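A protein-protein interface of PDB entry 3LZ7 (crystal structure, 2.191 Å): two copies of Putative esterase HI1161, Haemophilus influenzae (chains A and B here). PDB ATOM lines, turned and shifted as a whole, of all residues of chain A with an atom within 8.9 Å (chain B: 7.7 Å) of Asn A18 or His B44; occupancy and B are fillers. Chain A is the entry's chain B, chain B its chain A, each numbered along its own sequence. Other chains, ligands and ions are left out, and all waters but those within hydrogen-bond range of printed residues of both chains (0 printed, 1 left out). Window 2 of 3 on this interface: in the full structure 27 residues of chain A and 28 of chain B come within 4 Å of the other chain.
Of the printed residues of chain B, Asn A18 touches His B44.
Printed residues of chain B within 4 Å of Ala A20: His B44 (3.3 Å), Arg B45 (3.4 Å), Thr B46 (3.7 Å) and Met B47 (2.7 Å).
No residue of chain A comes within 4 Å of Asp B43.
Of chain A, only Asn A18 (3.3 Å), Ser A19 (3.1 Å) and Ala A20 (3.3 Å) come within 4 Å of His B44.
Of the printed residues of chain A, Arg B45 touches Ala A20 (3.4 Å) and His A23 (3.4 Å).
Printed residues of chain A within 4 Å of Pro B49: Leu A15 (3.2 Å).
The nearest residue of chain A that does not touch His B44 is His A23 (4.8 Å).
The nearest printed residue of chain B that does not touch His A23 is His B44 (4.8 Å).
The backbone NH of Ala A20 is in hydrogen-bond range of the backbone carbonyl oxygen of Met B47, at 2.7 Å.
O of His B44 lies within hydrogen-bond range of N of Ala A20, at 3.3 Å.
Of the 12 printed residues of chain A, 5 touch a printed residue of chain B.
Printed residues of chain A that touch a printed residue of chain B: Leu A15, Asn A18, Ser A19, Ala A20 and His A23.
Of the 9 printed residues of chain B, 5 touch a printed residue of chain A.
Hydrophobic or aromatic side chains of chain B that line the printed part of chain A: His B44 and Pro B49.
Among the printed residues, no Asp or Glu carboxylate lies within 4 Å of a Lys or Arg side-chain nitrogen of the other chain.
No position is printed for both chains.
The side-chain hydroxyl of Ser A22 sits at hydrogen-bond distance from the backbone NH of Ser A19.
OG of Ser A19 sits close to N of Val A21, at 3.1 Å.
The side-chain hydroxyl (OG1) of Thr B46 is in hydrogen-bond range of the backbone carbonyl oxygen (O) of Pro B41.
The backbone NH (N) of Asp B43 sits at hydrogen-bond distance from the side-chain hydroxyl (OG1) of Thr B46, at 3.0 Å.
The side-chain carboxylate (OD2) of Asp B43 lies within salt-bridge range of the guanidinium group (NH2) of Arg B45, 3.0 Å away.
The backbone NH (N) of Asn A18 lies within hydrogen-bond range of the side-chain hydroxyl (OG) of Ser A22.
Among the printed residues, pairs that only touch across the chains: Ser A19 with His B44, Leu A15 with Pro B49, Ser A19 with Met B47, Asn A18 with His B44, Ala A20 with Arg B45, His A23 with Arg B45 and Ala A20 with Thr B46.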
ATOM      1  N   ASN A  13     -22.881   5.583   2.219  1.00  0.00           N
ATOM      2  CA  ASN A  13     -21.506   5.890   2.616  1.00  0.00           C
ATOM      3  C   ASN A  13     -21.177   7.382   2.576  1.00  0.00           C
ATOM      4  O   ASN A  13     -20.402   7.863   3.398  1.00  0.00           O
ATOM      5  CB  ASN A  13     -20.490   5.060   1.831  1.00  0.00           C
ATOM      6  CG  ASN A  13     -20.361   3.637   2.374  1.00  0.00           C
ATOM      7  OD1 ASN A  13     -19.986   3.433   3.533  1.00  0.00           O
ATOM      8  ND2 ASN A  13     -20.681   2.653   1.542  1.00  0.00           N
ATOM      9  N   GLN A  14     -21.779   8.108   1.636  1.00  0.00           N
ATOM     10  CA  GLN A  14     -21.671   9.567   1.597  1.00  0.00           C
ATOM     11  C   GLN A  14     -22.362  10.240   2.790  1.00  0.00           C
ATOM     12  O   GLN A  14     -21.868  11.223   3.327  1.00  0.00           O
ATOM     13  CB  GLN A  14     -22.252  10.122   0.292  1.00  0.00           C
ATOM     14  CG  GLN A  14     -21.226  10.768  -0.626  1.00  0.00           C
ATOM     15  CD  GLN A  14     -20.411  11.853   0.072  1.00  0.00           C
ATOM     16  OE1 GLN A  14     -19.176  11.803   0.100  1.00  0.00           O
ATOM     17  NE2 GLN A  14     -21.100  12.833   0.648  1.00  0.00           N
ATOM     18  N   LEU A  15     -23.515   9.723   3.186  1.00  0.00           N
ATOM     19  CA  LEU A  15     -24.231  10.252   4.344  1.00  0.00           C
ATOM     20  C   LEU A  15     -23.377  10.168   5.618  1.00  0.00           C
ATOM     21  O   LEU A  15     -23.491  11.009   6.509  1.00  0.00           O
ATOM     22  CB  LEU A  15     -25.548   9.491   4.556  1.00  0.00           C
ATOM     23  CG  LEU A  15     -26.311   9.854   5.842  1.00  0.00           C
ATOM     24  CD1 LEU A  15     -27.051  11.185   5.689  1.00  0.00           C
ATOM     25  CD2 LEU A  15     -27.273   8.752   6.275  1.00  0.00           C
ATOM     26  N   CYS A  16     -22.528   9.142   5.683  1.00  0.00           N
ATOM     27  CA  CYS A  16     -21.714   8.852   6.861  1.00  0.00           C
ATOM     28  C   CYS A  16     -20.322   9.493   6.847  1.00  0.00           C
ATOM     29  O   CYS A  16     -19.567   9.347   7.803  1.00  0.00           O
ATOM     30  CB  CYS A  16     -21.560   7.334   7.041  1.00  0.00           C
ATOM     31  SG  CYS A  16     -23.068   6.459   7.491  1.00  0.00           S
ATOM     32  N   SER A  17     -19.973  10.183   5.769  1.00  0.00           N
ATOM     33  CA  SER A  17     -18.651  10.788   5.686  1.00  0.00           C
ATOM     34  C   SER A  17     -18.475  11.860   6.757  1.00  0.00           C
ATOM     35  O   SER A  17     -19.447  12.437   7.241  1.00  0.00           O
ATOM     36  CB  SER A  17     -18.399  11.361   4.285  1.00  0.00           C
ATOM     37  OG  SER A  17     -19.526  12.084   3.826  1.00  0.00           O
ATOM     38  N   ASN A  18     -17.228  12.116   7.128  1.00  0.00           N
ATOM     39  CA  ASN A  18     -16.913  13.092   8.167  1.00  0.00           C
ATOM     40  C   ASN A  18     -17.783  12.961   9.419  1.00  0.00           C
ATOM     41  O   ASN A  18     -18.300  13.946   9.939  1.00  0.00           O
ATOM     42  CB  ASN A  18     -16.955  14.522   7.615  1.00  0.00           C
ATOM     43  CG  ASN A  18     -16.309  15.525   8.555  1.00  0.00           C
ATOM     44  OD1 ASN A  18     -15.230  15.280   9.103  1.00  0.00           O
ATOM     45  ND2 ASN A  18     -16.966  16.665   8.745  1.00  0.00           N
ATOM     46  N   SER A  19     -17.941  11.730   9.890  1.00  0.00           N
ATOM     47  CA  SER A  19     -18.596  11.466  11.162  1.00  0.00           C
ATOM     48  C   SER A  19     -17.816  10.376  11.887  1.00  0.00           C
ATOM     49  O   SER A  19     -16.765   9.938  11.409  1.00  0.00           O
ATOM     50  CB  SER A  19     -20.046  11.031  10.946  1.00  0.00           C
ATOM     51  OG  SER A  19     -20.127   9.665  10.558  1.00  0.00           O
ATOM     52  N   ALA A  20     -18.330   9.949  13.038  1.00  0.00           N
ATOM     53  CA  ALA A  20     -17.732   8.859  13.796  1.00  0.00           C
ATOM     54  C   ALA A  20     -17.598   7.621  12.920  1.00  0.00           C
ATOM     55  O   ALA A  20     -16.648   6.853  13.055  1.00  0.00           O
ATOM     56  CB  ALA A  20     -18.572   8.545  15.021  1.00  0.00           C
ATOM     57  N   VAL A  21     -18.559   7.438  12.020  1.00  0.00           N
ATOM     58  CA  VAL A  21     -18.602   6.258  11.165  1.00  0.00           C
ATOM     59  C   VAL A  21     -17.385   6.204  10.227  1.00  0.00           C
ATOM     60  O   VAL A  21     -16.645   5.218  10.202  1.00  0.00           O
ATOM     61  CB  VAL A  21     -19.913   6.211  10.359  1.00  0.00           C
ATOM     62  CG1 VAL A  21     -19.981   4.972   9.484  1.00  0.00           C
ATOM     63  CG2 VAL A  21     -21.113   6.257  11.307  1.00  0.00           C
ATOM     64  N   SER A  22     -17.166   7.265   9.462  1.00  0.00           N
ATOM     65  CA  SER A  22     -15.983   7.299   8.613  1.00  0.00           C
ATOM     66  C   SER A  22     -14.717   7.352   9.467  1.00  0.00           C
ATOM     67  O   SER A  22     -13.698   6.754   9.120  1.00  0.00           O
ATOM     68  CB  SER A  22     -16.033   8.488   7.646  1.00  0.00           C
ATOM     69  OG  SER A  22     -16.169   9.705   8.354  1.00  0.00           O
ATOM     70  N   HIS A  23     -14.780   8.054  10.595  1.00  0.00           N
ATOM     71  CA  HIS A  23     -13.607   8.172  11.473  1.00  0.00           C
ATOM     72  C   HIS A  23     -13.097   6.794  11.931  1.00  0.00           C
ATOM     73  O   HIS A  23     -11.893   6.600  12.145  1.00  0.00           O
ATOM     74  CB  HIS A  23     -13.933   9.063  12.678  1.00  0.00           C
ATOM     75  CG  HIS A  23     -12.734   9.469  13.481  1.00  0.00           C
ATOM     76  ND1 HIS A  23     -11.683  10.180  12.944  1.00  0.00           N
ATOM     77  CD2 HIS A  23     -12.427   9.273  14.785  1.00  0.00           C
ATOM     78  CE1 HIS A  23     -10.774  10.397  13.878  1.00  0.00           C
ATOM     79  NE2 HIS A  23     -11.204   9.860  15.007  1.00  0.00           N
ATOM     80  N   LEU A  24     -14.013   5.835  12.056  1.00  0.00           N
ATOM     81  CA  LEU A  24     -13.645   4.471  12.464  1.00  0.00           C
ATOM     82  C   LEU A  24     -13.433   3.535  11.268  1.00  0.00           C
ATOM     83  O   LEU A  24     -13.302   2.328  11.438  1.00  0.00           O
ATOM     84  CB  LEU A  24     -14.717   3.878  13.393  1.00  0.00           C
ATOM     85  CG  LEU A  24     -14.858   4.592  14.740  1.00  0.00           C
ATOM     86  CD1 LEU A  24     -16.128   4.173  15.469  1.00  0.00           C
ATOM     87  CD2 LEU A  24     -13.622   4.337  15.593  1.00  0.00           C
ATOM     88  N   PRO B  41     -14.649  14.495  23.569  1.00  0.00           N
ATOM     89  CA  PRO B  41     -15.272  15.643  22.903  1.00  0.00           C
ATOM     90  C   PRO B  41     -16.464  15.190  22.074  1.00  0.00           C
ATOM     91  O   PRO B  41     -16.509  14.038  21.623  1.00  0.00           O
ATOM     92  CB  PRO B  41     -14.167  16.163  21.956  1.00  0.00           C
ATOM     93  CG  PRO B  41     -12.958  15.287  22.200  1.00  0.00           C
ATOM     94  CD  PRO B  41     -13.439  14.034  22.869  1.00  0.00           C
ATOM     95  N   VAL B  42     -17.433  16.079  21.886  1.00  0.00           N
ATOM     96  CA  VAL B  42     -18.508  15.816  20.940  1.00  0.00           C
ATOM     97  C   VAL B  42     -18.212  16.620  19.687  1.00  0.00           C
ATOM     98  O   VAL B  42     -18.410  17.827  19.659  1.00  0.00           O
ATOM     99  CB  VAL B  42     -19.886  16.187  21.501  1.00  0.00           C
ATOM    100  CG1 VAL B  42     -20.958  15.912  20.461  1.00  0.00           C
ATOM    101  CG2 VAL B  42     -20.163  15.388  22.765  1.00  0.00           C
ATOM    102  N   ASP B  43     -17.675  15.952  18.675  1.00  0.00           N
ATOM    103  CA  ASP B  43     -17.318  16.617  17.429  1.00  0.00           C
ATOM    104  C   ASP B  43     -17.386  15.629  16.271  1.00  0.00           C
ATOM    105  O   ASP B  43     -17.920  14.531  16.424  1.00  0.00           O
ATOM    106  CB  ASP B  43     -15.958  17.348  17.522  1.00  0.00           C
ATOM    107  CG  ASP B  43     -14.770  16.408  17.791  1.00  0.00           C
ATOM    108  OD1 ASP B  43     -14.797  15.229  17.392  1.00  0.00           O
ATOM    109  OD2 ASP B  43     -13.775  16.873  18.387  1.00  0.00           O
ATOM    110  N   HIS B  44     -16.869  16.028  15.116  1.00  0.00           N
ATOM    111  CA  HIS B  44     -16.971  15.211  13.914  1.00  0.00           C
ATOM    112  C   HIS B  44     -16.407  13.806  14.109  1.00  0.00           C
ATOM    113  O   HIS B  44     -16.796  12.889  13.400  1.00  0.00           O
ATOM    114  CB  HIS B  44     -16.271  15.898  12.734  1.00  0.00           C
ATOM    115  CG  HIS B  44     -14.786  15.696  12.716  1.00  0.00           C
ATOM    116  ND1 HIS B  44     -13.906  16.573  13.316  1.00  0.00           N
ATOM    117  CD2 HIS B  44     -14.026  14.712  12.177  1.00  0.00           C
ATOM    118  CE1 HIS B  44     -12.669  16.141  13.141  1.00  0.00           C
ATOM    119  NE2 HIS B  44     -12.714  15.012  12.455  1.00  0.00           N
ATOM    120  N   ARG B  45     -15.493  13.644  15.069  1.00  0.00           N
ATOM    121  CA  ARG B  45     -14.884  12.345  15.357  1.00  0.00           C
ATOM    122  C   ARG B  45     -15.826  11.417  16.099  1.00  0.00           C
ATOM    123  O   ARG B  45     -15.654  10.205  16.068  1.00  0.00           O
ATOM    124  CB  ARG B  45     -13.631  12.509  16.226  1.00  0.00           C
ATOM    125  CG  ARG B  45     -12.413  13.040  15.509  1.00  0.00           C
ATOM    126  CD  ARG B  45     -11.272  13.240  16.492  1.00  0.00           C
ATOM    127  NE  ARG B  45     -11.568  14.327  17.411  1.00  0.00           N
ATOM    128  CZ  ARG B  45     -10.764  14.721  18.391  1.00  0.00           C
ATOM    129  NH1 ARG B  45      -9.605  14.099  18.596  1.00  0.00           N
ATOM    130  NH2 ARG B  45     -11.121  15.739  19.168  1.00  0.00           N
ATOM    131  N   THR B  46     -16.807  11.988  16.788  1.00  0.00           N
ATOM    132  CA  THR B  46     -17.605  11.212  17.732  1.00  0.00           C
ATOM    133  C   THR B  46     -19.102  11.316  17.451  1.00  0.00           C
ATOM    134  O   THR B  46     -19.900  10.620  18.069  1.00  0.00           O
ATOM    135  CB  THR B  46     -17.313  11.644  19.171  1.00  0.00           C
ATOM    136  OG1 THR B  46     -17.505  13.060  19.302  1.00  0.00           O
ATOM    137  CG2 THR B  46     -15.861  11.292  19.545  1.00  0.00           C
ATOM    138  N   MET B  47     -19.474  12.179  16.506  1.00  0.00           N
ATOM    139  CA  MET B  47     -20.873  12.358  16.142  1.00  0.00           C
ATOM    140  C   MET B  47     -21.365  11.359  15.091  1.00  0.00           C
ATOM    141  O   MET B  47     -20.601  10.920  14.221  1.00  0.00           O
ATOM    142  CB  MET B  47     -21.093  13.778  15.614  1.00  0.00           C
ATOM    143  CG  MET B  47     -20.880  14.885  16.650  1.00  0.00           C
ATOM    144  SD  MET B  47     -20.958  16.712  15.867  1.00  0.00           S
ATOM    145  CE  MET B  47     -20.093  16.356  14.158  1.00  0.00           C
ATOM    146  N   GLN B  48     -22.649  11.010  15.179  1.00  0.00           N
ATOM    147  CA  GLN B  48     -23.364  10.365  14.074  1.00  0.00           C
ATOM    148  C   GLN B  48     -23.693  11.421  13.013  1.00  0.00           C
ATOM    149  O   GLN B  48     -23.541  12.628  13.262  1.00  0.00           O
ATOM    150  CB  GLN B  48     -24.641   9.706  14.581  1.00  0.00           C
ATOM    151  CG  GLN B  48     -25.663  10.706  15.044  1.00  0.00           C
ATOM    152  CD  GLN B  48     -26.822  10.056  15.735  1.00  0.00           C
ATOM    153  OE1 GLN B  48     -27.966  10.486  15.593  1.00  0.00           O
ATOM    154  NE2 GLN B  48     -26.539   9.010  16.497  1.00  0.00           N
ATOM    155  N   PRO B  49     -24.133  10.980  11.819  1.00  0.00           N
ATOM    156  CA  PRO B  49     -24.212  11.924  10.699  1.00  0.00           C
ATOM    157  C   PRO B  49     -25.190  13.091  10.883  1.00  0.00           C
ATOM    158  O   PRO B  49     -25.354  13.854   9.936  1.00  0.00           O
ATOM    159  CB  PRO B  49     -24.643  11.043   9.522  1.00  0.00           C
ATOM    160  CG  PRO B  49     -24.188   9.679   9.895  1.00  0.00           C
ATOM    161  CD  PRO B  49     -24.362   9.591  11.381  1.00  0.00           C
